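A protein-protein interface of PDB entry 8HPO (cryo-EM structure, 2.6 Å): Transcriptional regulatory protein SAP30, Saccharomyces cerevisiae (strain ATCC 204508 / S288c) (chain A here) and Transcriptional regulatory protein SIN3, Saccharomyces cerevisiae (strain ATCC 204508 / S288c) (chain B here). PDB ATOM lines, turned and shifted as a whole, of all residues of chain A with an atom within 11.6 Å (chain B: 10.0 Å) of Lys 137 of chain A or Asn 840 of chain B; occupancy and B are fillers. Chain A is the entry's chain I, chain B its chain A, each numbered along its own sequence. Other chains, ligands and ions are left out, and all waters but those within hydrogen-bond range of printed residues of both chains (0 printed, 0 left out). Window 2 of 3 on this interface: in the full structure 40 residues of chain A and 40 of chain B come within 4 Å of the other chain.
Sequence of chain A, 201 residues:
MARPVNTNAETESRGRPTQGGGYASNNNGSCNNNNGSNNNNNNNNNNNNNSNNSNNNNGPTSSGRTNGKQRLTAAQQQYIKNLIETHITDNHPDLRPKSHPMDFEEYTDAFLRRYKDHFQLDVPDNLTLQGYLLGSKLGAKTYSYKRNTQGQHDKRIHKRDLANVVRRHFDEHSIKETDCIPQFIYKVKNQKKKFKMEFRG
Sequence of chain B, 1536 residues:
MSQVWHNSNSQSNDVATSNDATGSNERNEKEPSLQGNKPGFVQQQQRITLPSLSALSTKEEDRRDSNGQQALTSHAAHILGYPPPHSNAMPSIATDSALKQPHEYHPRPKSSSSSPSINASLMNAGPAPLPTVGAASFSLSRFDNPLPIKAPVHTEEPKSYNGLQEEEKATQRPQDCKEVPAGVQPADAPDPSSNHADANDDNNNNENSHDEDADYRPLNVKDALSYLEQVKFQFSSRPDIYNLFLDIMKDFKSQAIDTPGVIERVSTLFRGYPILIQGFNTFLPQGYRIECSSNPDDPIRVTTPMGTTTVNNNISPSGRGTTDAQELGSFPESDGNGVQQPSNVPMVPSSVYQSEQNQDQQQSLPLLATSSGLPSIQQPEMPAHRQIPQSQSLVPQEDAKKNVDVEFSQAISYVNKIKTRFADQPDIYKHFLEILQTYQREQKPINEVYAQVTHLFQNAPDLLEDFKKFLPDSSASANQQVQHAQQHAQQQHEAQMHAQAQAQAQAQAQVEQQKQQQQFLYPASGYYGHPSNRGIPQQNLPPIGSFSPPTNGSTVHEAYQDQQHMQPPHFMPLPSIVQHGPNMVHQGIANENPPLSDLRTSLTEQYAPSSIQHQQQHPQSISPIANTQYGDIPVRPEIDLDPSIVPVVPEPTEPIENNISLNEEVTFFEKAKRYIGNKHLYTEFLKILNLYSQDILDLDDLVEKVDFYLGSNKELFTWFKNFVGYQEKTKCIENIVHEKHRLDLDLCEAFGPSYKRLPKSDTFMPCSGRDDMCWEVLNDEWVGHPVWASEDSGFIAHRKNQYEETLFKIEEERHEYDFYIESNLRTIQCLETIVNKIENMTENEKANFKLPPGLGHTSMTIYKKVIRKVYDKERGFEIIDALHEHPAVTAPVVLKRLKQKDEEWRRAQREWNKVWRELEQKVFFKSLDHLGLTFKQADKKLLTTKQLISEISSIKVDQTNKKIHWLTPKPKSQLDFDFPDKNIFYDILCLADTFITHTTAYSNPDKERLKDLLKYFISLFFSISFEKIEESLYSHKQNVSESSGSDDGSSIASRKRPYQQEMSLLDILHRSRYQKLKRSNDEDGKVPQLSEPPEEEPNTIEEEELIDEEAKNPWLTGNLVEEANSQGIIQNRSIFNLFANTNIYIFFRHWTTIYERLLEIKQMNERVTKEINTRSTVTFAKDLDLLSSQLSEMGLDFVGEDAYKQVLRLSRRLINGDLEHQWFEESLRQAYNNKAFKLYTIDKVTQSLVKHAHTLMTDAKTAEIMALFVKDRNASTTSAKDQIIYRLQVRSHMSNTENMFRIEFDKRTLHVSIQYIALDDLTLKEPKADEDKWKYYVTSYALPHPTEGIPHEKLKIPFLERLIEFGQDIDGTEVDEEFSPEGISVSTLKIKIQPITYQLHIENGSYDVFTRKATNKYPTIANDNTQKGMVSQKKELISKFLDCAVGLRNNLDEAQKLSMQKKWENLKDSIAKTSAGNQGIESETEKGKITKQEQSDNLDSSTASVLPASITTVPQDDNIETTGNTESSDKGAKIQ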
ATOM      1  N   LEU A 127     -12.310 -11.319  27.517  1.00  0.00           N
ATOM      2  CA  LEU A 127     -11.198 -11.039  26.617  1.00  0.00           C
ATOM      3  C   LEU A 127     -11.062  -9.527  26.482  1.00  0.00           C
ATOM      4  O   LEU A 127     -12.051  -8.842  26.205  1.00  0.00           O
ATOM      5  CB  LEU A 127     -11.445 -11.675  25.251  1.00  0.00           C
ATOM      6  CG  LEU A 127     -11.186 -13.163  25.038  1.00  0.00           C
ATOM      7  CD1 LEU A 127     -11.462 -13.509  23.603  1.00  0.00           C
ATOM      8  CD2 LEU A 127      -9.776 -13.526  25.410  1.00  0.00           C
ATOM      9  N   GLY A 131      -6.992  -9.561  23.004  1.00  0.00           N
ATOM     10  CA  GLY A 131      -7.351 -10.950  22.837  1.00  0.00           C
ATOM     11  C   GLY A 131      -8.550 -11.182  21.973  1.00  0.00           C
ATOM     12  O   GLY A 131      -8.767 -12.308  21.526  1.00  0.00           O
ATOM     13  N   TYR A 132      -9.338 -10.147  21.716  1.00  0.00           N
ATOM     14  CA  TYR A 132     -10.500 -10.301  20.855  1.00  0.00           C
ATOM     15  C   TYR A 132     -10.191  -9.988  19.398  1.00  0.00           C
ATOM     16  O   TYR A 132     -10.846 -10.529  18.502  1.00  0.00           O
ATOM     17  CB  TYR A 132     -11.637  -9.411  21.340  1.00  0.00           C
ATOM     18  CG  TYR A 132     -12.825  -9.439  20.423  1.00  0.00           C
ATOM     19  CD1 TYR A 132     -13.473 -10.629  20.137  1.00  0.00           C
ATOM     20  CD2 TYR A 132     -13.293  -8.282  19.832  1.00  0.00           C
ATOM     21  CE1 TYR A 132     -14.553 -10.663  19.296  1.00  0.00           C
ATOM     22  CE2 TYR A 132     -14.379  -8.305  18.990  1.00  0.00           C
ATOM     23  CZ  TYR A 132     -15.004  -9.497  18.723  1.00  0.00           C
ATOM     24  OH  TYR A 132     -16.088  -9.523  17.882  1.00  0.00           O
ATOM     25  N   LEU A 133      -9.214  -9.123  19.132  1.00  0.00           N
ATOM     26  CA  LEU A 133      -8.729  -8.927  17.773  1.00  0.00           C
ATOM     27  C   LEU A 133      -7.651  -9.929  17.403  1.00  0.00           C
ATOM     28  O   LEU A 133      -7.327 -10.066  16.221  1.00  0.00           O
ATOM     29  CB  LEU A 133      -8.196  -7.506  17.583  1.00  0.00           C
ATOM     30  CG  LEU A 133      -9.116  -6.345  17.944  1.00  0.00           C
ATOM     31  CD1 LEU A 133      -8.309  -5.078  18.081  1.00  0.00           C
ATOM     32  CD2 LEU A 133     -10.196  -6.177  16.908  1.00  0.00           C
ATOM     33  N   LEU A 134      -7.098 -10.625  18.383  1.00  0.00           N
ATOM     34  CA  LEU A 134      -6.177 -11.731  18.183  1.00  0.00           C
ATOM     35  C   LEU A 134      -6.849 -12.951  17.571  1.00  0.00           C
ATOM     36  O   LEU A 134      -6.186 -13.971  17.371  1.00  0.00           O
ATOM     37  CB  LEU A 134      -5.541 -12.107  19.520  1.00  0.00           C
ATOM     38  CG  LEU A 134      -4.286 -12.961  19.577  1.00  0.00           C
ATOM     39  CD1 LEU A 134      -3.167 -12.287  18.840  1.00  0.00           C
ATOM     40  CD2 LEU A 134      -3.918 -13.138  21.009  1.00  0.00           C
ATOM     41  N   GLY A 135      -8.135 -12.874  17.258  1.00  0.00           N
ATOM     42  CA  GLY A 135      -8.821 -14.018  16.701  1.00  0.00           C
ATOM     43  C   GLY A 135      -9.018 -13.898  15.210  1.00  0.00           C
ATOM     44  O   GLY A 135      -9.890 -13.168  14.735  1.00  0.00           O
ATOM     45  N   SER A 136      -8.200 -14.634  14.470  1.00  0.00           N
ATOM     46  CA  SER A 136      -8.206 -14.655  13.016  1.00  0.00           C
ATOM     47  C   SER A 136      -7.423 -15.890  12.609  1.00  0.00           C
ATOM     48  O   SER A 136      -6.756 -16.517  13.434  1.00  0.00           O
ATOM     49  CB  SER A 136      -7.591 -13.388  12.426  1.00  0.00           C
ATOM     50  OG  SER A 136      -6.486 -12.956  13.201  1.00  0.00           O
ATOM     51  N   LYS A 137      -7.514 -16.241  11.327  1.00  0.00           N
ATOM     52  CA  LYS A 137      -6.814 -17.425  10.846  1.00  0.00           C
ATOM     53  C   LYS A 137      -5.317 -17.328  11.102  1.00  0.00           C
ATOM     54  O   LYS A 137      -4.659 -18.338  11.371  1.00  0.00           O
ATOM     55  CB  LYS A 137      -7.090 -17.628   9.361  1.00  0.00           C
ATOM     56  CG  LYS A 137      -8.375 -18.357   9.077  1.00  0.00           C
ATOM     57  CD  LYS A 137      -9.482 -17.386   8.740  1.00  0.00           C
ATOM     58  CE  LYS A 137     -10.646 -18.094   8.076  1.00  0.00           C
ATOM     59  NZ  LYS A 137     -11.772 -17.168   7.787  1.00  0.00           N
ATOM     60  N   LEU A 138      -4.761 -16.120  11.033  1.00  0.00           N
ATOM     61  CA  LEU A 138      -3.353 -15.938  11.365  1.00  0.00           C
ATOM     62  C   LEU A 138      -3.151 -15.887  12.871  1.00  0.00           C
ATOM     63  O   LEU A 138      -2.230 -16.518  13.397  1.00  0.00           O
ATOM     64  CB  LEU A 138      -2.822 -14.667  10.698  1.00  0.00           C
ATOM     65  CG  LEU A 138      -1.314 -14.428  10.571  1.00  0.00           C
ATOM     66  CD1 LEU A 138      -0.766 -13.660  11.748  1.00  0.00           C
ATOM     67  CD2 LEU A 138      -0.568 -15.734  10.405  1.00  0.00           C
ATOM     68  N   GLY A 139      -4.015 -15.160  13.578  1.00  0.00           N
ATOM     69  CA  GLY A 139      -3.952 -15.072  15.025  1.00  0.00           C
ATOM     70  C   GLY A 139      -4.272 -16.358  15.755  1.00  0.00           C
ATOM     71  O   GLY A 139      -3.956 -16.463  16.943  1.00  0.00           O
ATOM     72  N   ALA A 140      -4.866 -17.333  15.078  1.00  0.00           N
ATOM     73  CA  ALA A 140      -5.259 -18.599  15.678  1.00  0.00           C
ATOM     74  C   ALA A 140      -4.089 -19.529  15.957  1.00  0.00           C
ATOM     75  O   ALA A 140      -4.319 -20.687  16.312  1.00  0.00           O
ATOM     76  CB  ALA A 140      -6.267 -19.314  14.780  1.00  0.00           C
ATOM     77  N   LYS A 141      -2.852 -19.069  15.806  1.00  0.00           N
ATOM     78  CA  LYS A 141      -1.676 -19.889  16.052  1.00  0.00           C
ATOM     79  C   LYS A 141      -0.836 -19.355  17.198  1.00  0.00           C
ATOM     80  O   LYS A 141       0.244 -19.888  17.468  1.00  0.00           O
ATOM     81  CB  LYS A 141      -0.833 -19.986  14.786  1.00  0.00           C
ATOM     82  CG  LYS A 141      -1.633 -19.743  13.522  1.00  0.00           C
ATOM     83  CD  LYS A 141      -0.786 -19.917  12.288  1.00  0.00           C
ATOM     84  CE  LYS A 141      -1.646 -20.212  11.081  1.00  0.00           C
ATOM     85  NZ  LYS A 141      -0.817 -20.321   9.856  1.00  0.00           N
ATOM     86  N   THR A 142      -1.304 -18.316  17.872  1.00  0.00           N
ATOM     87  CA  THR A 142      -0.634 -17.745  19.026  1.00  0.00           C
ATOM     88  C   THR A 142      -0.994 -18.525  20.284  1.00  0.00           C
ATOM     89  O   THR A 142      -2.032 -19.178  20.369  1.00  0.00           O
ATOM     90  CB  THR A 142      -1.015 -16.274  19.186  1.00  0.00           C
ATOM     91  OG1 THR A 142      -2.426 -16.129  19.006  1.00  0.00           O
ATOM     92  CG2 THR A 142      -0.319 -15.440  18.147  1.00  0.00           C
ATOM     93  N   TYR A 143      -0.106 -18.438  21.275  1.00  0.00           N
ATOM     94  CA  TYR A 143      -0.320 -19.115  22.549  1.00  0.00           C
ATOM     95  C   TYR A 143      -1.617 -18.681  23.218  1.00  0.00           C
ATOM     96  O   TYR A 143      -2.241 -19.480  23.921  1.00  0.00           O
ATOM     97  CB  TYR A 143       0.884 -18.858  23.454  1.00  0.00           C
ATOM     98  CG  TYR A 143       0.742 -19.242  24.910  1.00  0.00           C
ATOM     99  CD1 TYR A 143       0.072 -18.420  25.810  1.00  0.00           C
ATOM    100  CD2 TYR A 143       1.320 -20.403  25.396  1.00  0.00           C
ATOM    101  CE1 TYR A 143      -0.039 -18.759  27.136  1.00  0.00           C
ATOM    102  CE2 TYR A 143       1.213 -20.746  26.724  1.00  0.00           C
ATOM    103  CZ  TYR A 143       0.534 -19.921  27.588  1.00  0.00           C
ATOM    104  OH  TYR A 143       0.423 -20.263  28.912  1.00  0.00           O
ATOM    105  N   TYR A 145      -4.626 -17.700  21.819  1.00  0.00           N
ATOM    106  CA  TYR A 145      -5.737 -18.418  21.208  1.00  0.00           C
ATOM    107  C   TYR A 145      -5.762 -19.874  21.656  1.00  0.00           C
ATOM    108  O   TYR A 145      -6.808 -20.397  22.056  1.00  0.00           O
ATOM    109  CB  TYR A 145      -5.629 -18.319  19.693  1.00  0.00           C
ATOM    110  CG  TYR A 145      -6.933 -18.450  18.964  1.00  0.00           C
ATOM    111  CD1 TYR A 145      -7.380 -19.681  18.525  1.00  0.00           C
ATOM    112  CD2 TYR A 145      -7.711 -17.342  18.698  1.00  0.00           C
ATOM    113  CE1 TYR A 145      -8.569 -19.804  17.849  1.00  0.00           C
ATOM    114  CE2 TYR A 145      -8.904 -17.457  18.023  1.00  0.00           C
ATOM    115  CZ  TYR A 145      -9.325 -18.690  17.602  1.00  0.00           C
ATOM    116  OH  TYR A 145     -10.513 -18.804  16.930  1.00  0.00           O
ATOM    117  N   LYS A 146      -4.609 -20.541  21.618  1.00  0.00           N
ATOM    118  CA  LYS A 146      -4.577 -21.964  21.924  1.00  0.00           C
ATOM    119  C   LYS A 146      -4.609 -22.226  23.421  1.00  0.00           C
ATOM    120  O   LYS A 146      -4.632 -23.386  23.842  1.00  0.00           O
ATOM    121  CB  LYS A 146      -3.341 -22.611  21.307  1.00  0.00           C
ATOM    122  CG  LYS A 146      -3.077 -22.217  19.874  1.00  0.00           C
ATOM    123  CD  LYS A 146      -2.198 -23.235  19.188  1.00  0.00           C
ATOM    124  CE  LYS A 146      -0.837 -23.308  19.840  1.00  0.00           C
ATOM    125  NZ  LYS A 146       0.246 -23.401  18.828  1.00  0.00           N
ATOM    126  N   THR A 149      -9.016 -21.214  23.819  1.00  0.00           N
ATOM    127  CA  THR A 149     -10.038 -21.773  22.946  1.00  0.00           C
ATOM    128  C   THR A 149     -10.095 -23.292  22.934  1.00  0.00           C
ATOM    129  O   THR A 149     -11.067 -23.846  22.409  1.00  0.00           O
ATOM    130  CB  THR A 149      -9.844 -21.286  21.503  1.00  0.00           C
ATOM    131  OG1 THR A 149     -11.117 -21.220  20.853  1.00  0.00           O
ATOM    132  CG2 THR A 149      -8.944 -22.241  20.733  1.00  0.00           C
ATOM    133  N   GLU B 832      -4.743  -3.355   8.911  1.00  0.00           N
ATOM    134  CA  GLU B 832      -4.507  -4.712   8.438  1.00  0.00           C
ATOM    135  C   GLU B 832      -4.848  -5.736   9.506  1.00  0.00           C
ATOM    136  O   GLU B 832      -5.507  -6.741   9.214  1.00  0.00           O
ATOM    137  CB  GLU B 832      -3.057  -4.878   7.995  1.00  0.00           C
ATOM    138  CG  GLU B 832      -2.904  -5.446   6.602  1.00  0.00           C
ATOM    139  CD  GLU B 832      -1.457  -5.729   6.249  1.00  0.00           C
ATOM    140  OE1 GLU B 832      -0.565  -5.091   6.847  1.00  0.00           O
ATOM    141  OE2 GLU B 832      -1.212  -6.594   5.379  1.00  0.00           O
ATOM    142  N   THR B 833      -4.392  -5.521  10.742  1.00  0.00           N
ATOM    143  CA  THR B 833      -4.810  -6.441  11.801  1.00  0.00           C
ATOM    144  C   THR B 833      -6.331  -6.478  11.932  1.00  0.00           C
ATOM    145  O   THR B 833      -6.929  -7.556  12.077  1.00  0.00           O
ATOM    146  CB  THR B 833      -4.171  -6.069  13.136  1.00  0.00           C
ATOM    147  OG1 THR B 833      -3.335  -4.923  12.968  1.00  0.00           O
ATOM    148  CG2 THR B 833      -3.345  -7.223  13.660  1.00  0.00           C
ATOM    149  N   ILE B 834      -6.977  -5.316  11.843  1.00  0.00           N
ATOM    150  CA  ILE B 834      -8.425  -5.274  12.049  1.00  0.00           C
ATOM    151  C   ILE B 834      -9.163  -6.008  10.930  1.00  0.00           C
ATOM    152  O   ILE B 834     -10.170  -6.682  11.173  1.00  0.00           O
ATOM    153  CB  ILE B 834      -8.896  -3.815  12.195  1.00  0.00           C
ATOM    154  CG1 ILE B 834      -8.619  -3.327  13.613  1.00  0.00           C
ATOM    155  CG2 ILE B 834     -10.369  -3.674  11.866  1.00  0.00           C
ATOM    156  CD1 ILE B 834      -8.591  -1.838  13.753  1.00  0.00           C
ATOM    157  N   VAL B 835      -8.661  -5.929   9.696  1.00  0.00           N
ATOM    158  CA  VAL B 835      -9.327  -6.620   8.592  1.00  0.00           C
ATOM    159  C   VAL B 835      -9.078  -8.120   8.667  1.00  0.00           C
ATOM    160  O   VAL B 835      -9.979  -8.928   8.400  1.00  0.00           O
ATOM    161  CB  VAL B 835      -8.869  -6.037   7.243  1.00  0.00           C
ATOM    162  CG1 VAL B 835      -9.370  -6.880   6.097  1.00  0.00           C
ATOM    163  CG2 VAL B 835      -9.384  -4.650   7.087  1.00  0.00           C
ATOM    164  N   ASN B 836      -7.854  -8.521   9.015  1.00  0.00           N
ATOM    165  CA  ASN B 836      -7.584  -9.937   9.236  1.00  0.00           C
ATOM    166  C   ASN B 836      -8.520 -10.523  10.278  1.00  0.00           C
ATOM    167  O   ASN B 836      -8.936 -11.679  10.156  1.00  0.00           O
ATOM    168  CB  ASN B 836      -6.137 -10.144   9.674  1.00  0.00           C
ATOM    169  CG  ASN B 836      -5.228 -10.479   8.525  1.00  0.00           C
ATOM    170  OD1 ASN B 836      -5.245  -9.811   7.494  1.00  0.00           O
ATOM    171  ND2 ASN B 836      -4.427 -11.523   8.687  1.00  0.00           N
ATOM    172  N   LYS B 837      -8.867  -9.748  11.308  1.00  0.00           N
ATOM    173  CA  LYS B 837      -9.791 -10.266  12.310  1.00  0.00           C
ATOM    174  C   LYS B 837     -11.234 -10.240  11.816  1.00  0.00           C
ATOM    175  O   LYS B 837     -12.015 -11.138  12.140  1.00  0.00           O
ATOM    176  CB  LYS B 837      -9.657  -9.481  13.610  1.00  0.00           C
ATOM    177  CG  LYS B 837     -10.593  -9.948  14.706  1.00  0.00           C
ATOM    178  CD  LYS B 837     -11.741  -8.981  14.893  1.00  0.00           C
ATOM    179  CE  LYS B 837     -12.982  -9.694  15.370  1.00  0.00           C
ATOM    180  NZ  LYS B 837     -14.202  -8.928  15.022  1.00  0.00           N
ATOM    181  N   ILE B 838     -11.614  -9.223  11.040  1.00  0.00           N
ATOM    182  CA  ILE B 838     -12.987  -9.147  10.545  1.00  0.00           C
ATOM    183  C   ILE B 838     -13.289 -10.284   9.579  1.00  0.00           C
ATOM    184  O   ILE B 838     -14.426 -10.765   9.508  1.00  0.00           O
ATOM    185  CB  ILE B 838     -13.247  -7.778   9.892  1.00  0.00           C
ATOM    186  CG1 ILE B 838     -13.396  -6.704  10.960  1.00  0.00           C
ATOM    187  CG2 ILE B 838     -14.487  -7.811   9.016  1.00  0.00           C
ATOM    188  CD1 ILE B 838     -13.514  -5.328  10.396  1.00  0.00           C
ATOM    189  N   GLU B 839     -12.286 -10.749   8.837  1.00  0.00           N
ATOM    190  CA  GLU B 839     -12.542 -11.829   7.888  1.00  0.00           C
ATOM    191  C   GLU B 839     -12.786 -13.176   8.559  1.00  0.00           C
ATOM    192  O   GLU B 839     -13.103 -14.143   7.860  1.00  0.00           O
ATOM    193  CB  GLU B 839     -11.377 -11.972   6.905  1.00  0.00           C
ATOM    194  CG  GLU B 839     -11.166 -10.787   5.977  1.00  0.00           C
ATOM    195  CD  GLU B 839      -9.831 -10.862   5.254  1.00  0.00           C
ATOM    196  OE1 GLU B 839      -9.215 -11.949   5.261  1.00  0.00           O
ATOM    197  OE2 GLU B 839      -9.398  -9.842   4.681  1.00  0.00           O
ATOM    198  N   ASN B 840     -12.647 -13.269   9.878  1.00  0.00           N
ATOM    199  CA  ASN B 840     -12.779 -14.518  10.622  1.00  0.00           C
ATOM    200  C   ASN B 840     -13.862 -14.383  11.683  1.00  0.00           C
ATOM    201  O   ASN B 840     -13.685 -14.743  12.846  1.00  0.00           O
ATOM    202  CB  ASN B 840     -11.440 -14.904  11.242  1.00  0.00           C
ATOM    203  CG  ASN B 840     -11.475 -16.245  11.937  1.00  0.00           C
ATOM    204  OD1 ASN B 840     -11.699 -17.275  11.312  1.00  0.00           O
ATOM    205  ND2 ASN B 840     -11.245 -16.238  13.241  1.00  0.00           N
ATOM    206  N   MET B 841     -15.009 -13.837  11.296  1.00  0.00           N
ATOM    207  CA  MET B 841     -16.065 -13.622  12.271  1.00  0.00           C
ATOM    208  C   MET B 841     -17.415 -13.616  11.574  1.00  0.00           C
ATOM    209  O   MET B 841     -17.506 -13.396  10.365  1.00  0.00           O
ATOM    210  CB  MET B 841     -15.838 -12.327  13.055  1.00  0.00           C
ATOM    211  CG  MET B 841     -16.425 -11.074  12.448  1.00  0.00           C
ATOM    212  SD  MET B 841     -15.959  -9.672  13.473  1.00  0.00           S
ATOM    213  CE  MET B 841     -16.613  -8.307  12.544  1.00  0.00           C
ATOM    214  N   THR B 842     -18.459 -13.855  12.363  1.00  0.00           N
ATOM    215  CA  THR B 842     -19.793 -14.112  11.845  1.00  0.00           C
ATOM    216  C   THR B 842     -20.472 -12.806  11.454  1.00  0.00           C
ATOM    217  O   THR B 842     -19.850 -11.747  11.378  1.00  0.00           O
ATOM    218  CB  THR B 842     -20.629 -14.851  12.882  1.00  0.00           C
ATOM    219  OG1 THR B 842     -21.227 -13.898  13.769  1.00  0.00           O
ATOM    220  CG2 THR B 842     -19.755 -15.793  13.685  1.00  0.00           C
ATOM    221  N   GLU B 843     -21.774 -12.887  11.194  1.00  0.00           N
ATOM    222  CA  GLU B 843     -22.512 -11.709  10.755  1.00  0.00           C
ATOM    223  C   GLU B 843     -23.052 -10.903  11.929  1.00  0.00           C
ATOM    224  O   GLU B 843     -23.088  -9.667  11.864  1.00  0.00           O
ATOM    225  CB  GLU B 843     -23.652 -12.127   9.828  1.00  0.00           C
ATOM    226  CG  GLU B 843     -24.095 -11.046   8.863  1.00  0.00           C
ATOM    227  CD  GLU B 843     -23.210 -10.959   7.634  1.00  0.00           C
ATOM    228  OE1 GLU B 843     -23.437 -10.059   6.799  1.00  0.00           O
ATOM    229  OE2 GLU B 843     -22.287 -11.789   7.500  1.00  0.00           O
ATOM    230  N   GLU B 845     -21.526 -10.758  14.808  1.00  0.00           N
ATOM    231  CA  GLU B 845     -20.326 -10.053  15.236  1.00  0.00           C
ATOM    232  C   GLU B 845     -19.952  -8.929  14.285  1.00  0.00           C
ATOM    233  O   GLU B 845     -19.216  -8.023  14.678  1.00  0.00           O
ATOM    234  CB  GLU B 845     -19.149 -11.013  15.366  1.00  0.00           C
ATOM    235  CG  GLU B 845     -19.279 -12.019  16.471  1.00  0.00           C
ATOM    236  CD  GLU B 845     -17.985 -12.751  16.719  1.00  0.00           C
ATOM    237  OE1 GLU B 845     -17.018 -12.110  17.180  1.00  0.00           O
ATOM    238  OE2 GLU B 845     -17.929 -13.965  16.445  1.00  0.00           O
ATOM    239  N   LYS B 846     -20.429  -8.969  13.042  1.00  0.00           N
ATOM    240  CA  LYS B 846     -20.176  -7.864  12.128  1.00  0.00           C
ATOM    241  C   LYS B 846     -21.102  -6.694  12.417  1.00  0.00           C
ATOM    242  O   LYS B 846     -20.708  -5.535  12.267  1.00  0.00           O
ATOM    243  CB  LYS B 846     -20.328  -8.324  10.679  1.00  0.00           C
ATOM    244  CG  LYS B 846     -19.061  -8.906  10.081  1.00  0.00           C
ATOM    245  CD  LYS B 846     -19.256  -9.314   8.635  1.00  0.00           C
ATOM    246  CE  LYS B 846     -18.136 -10.227   8.182  1.00  0.00           C
ATOM    247  NZ  LYS B 846     -18.303 -10.666   6.775  1.00  0.00           N
ATOM    248  N   PHE B 849     -19.823  -4.945  16.224  1.00  0.00           N
ATOM    249  CA  PHE B 849     -18.420  -4.598  16.368  1.00  0.00           C
ATOM    250  C   PHE B 849     -18.298  -3.089  16.494  1.00  0.00           C
ATOM    251  O   PHE B 849     -18.985  -2.346  15.786  1.00  0.00           O
ATOM    252  CB  PHE B 849     -17.604  -5.102  15.179  1.00  0.00           C
ATOM    253  CG  PHE B 849     -16.126  -5.088  15.408  1.00  0.00           C
ATOM    254  CD1 PHE B 849     -15.254  -4.877  14.359  1.00  0.00           C
ATOM    255  CD2 PHE B 849     -15.607  -5.284  16.669  1.00  0.00           C
ATOM    256  CE1 PHE B 849     -13.899  -4.861  14.563  1.00  0.00           C
ATOM    257  CE2 PHE B 849     -14.249  -5.272  16.875  1.00  0.00           C
ATOM    258  CZ  PHE B 849     -13.396  -5.061  15.821  1.00  0.00           C
ATOM    259  N   ALA B 888     -16.652  -2.767  10.631  1.00  0.00           N
ATOM    260  CA  ALA B 888     -16.765  -3.921   9.748  1.00  0.00           C
ATOM    261  C   ALA B 888     -17.155  -3.526   8.332  1.00  0.00           C
ATOM    262  O   ALA B 888     -16.774  -4.202   7.374  1.00  0.00           O
ATOM    263  CB  ALA B 888     -17.774  -4.918  10.313  1.00  0.00           C
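Of the printed residues of chain B, Tyr 132 of chain A touches Lys 837, Glu 845 and Phe 849.
Lys 137 of chain A touches just these residues of chain B: Glu 839 and Asn 840.
No residue of chain B comes within 4 Å of Leu 138 of chain A.
No residue of chain B comes within 4 Å of Ala 140 of chain A.
Ile 834 of chain B touches none of the printed residues of chain A.
Lys 837 of chain B touches four residues of chain A.
Of chain A, only Lys 137 (3.3 Å) comes within 4 Å of Glu 839 of chain B.
Of chain A, only Gly 135, Ser 136 and Lys 137 come within 4 Å of Asn 840 of chain B.
No residue of chain A comes within 4 Å of Met 841 of chain B.
Of the printed residues of chain A, Phe 849 of chain B touches Tyr 132 and Leu 133.
The nearest printed residue of chain A that does not touch Phe 849 of chain B is Leu 134 of chain A (8.8 Å).
The side-chain amino group (NZ) of Lys 837 of chain B sits at hydrogen-bond distance from the side-chain hydroxyl (OH) of Tyr 132 of chain A, 3.5 Å away.
The side-chain hydroxyl of Tyr 132 of chain A sits at hydrogen-bond distance from the side-chain carboxylate of Glu 845 of chain B (2.8 Å).
The side-chain amino group (NZ) of Lys 137 of chain A is in hydrogen-bond range of the backbone carbonyl oxygen (O) of Glu 839 of chain B, at 3.3 Å.
Printed residues of chain B that touch a printed residue of chain A: Asn 836, Lys 837, Glu 839, Asn 840, Glu 845 and Phe 849.
Hydrophobic or aromatic side chains of chain B that line the printed part of chain A: Phe 849.
Among the printed residues, pairs that only touch across the chains: Tyr 132 of chain A with Phe 849 of chain B (3.7 Å), Leu 133 of chain A with Lys 837 of chain B (3.5 Å), Leu 133 of chain A with Phe 849 of chain B (3.6 Å), Gly 135 of chain A with Lys 837 of chain B (3.3 Å), Gly 135 of chain A with Asn 840 of chain B (3.7 Å), Ser 136 of chain A with Asn 836 of chain B (3.1 Å), Ser 136 of chain A with Lys 837 of chain B (3.8 Å), Ser 136 of chain A with Asn 840 of chain B (3.4 Å) and Lys 137 of chain A with Asn 840 of chain B (3.4 Å).
OG of Ser 136 of chain A is in hydrogen-bond range of N of Gly 139 of chain A (3.3 Å).
The side-chain amino group (NZ) of Lys 837 of chain B lies within hydrogen-bond range of the side-chain sulfur (SD) of Met 841 of chain B, at 2.5 Å.
The side-chain hydroxyl of Thr 842 of chain B is in hydrogen-bond range of the backbone NH of Glu 845 of chain B, at 3.3 Å.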
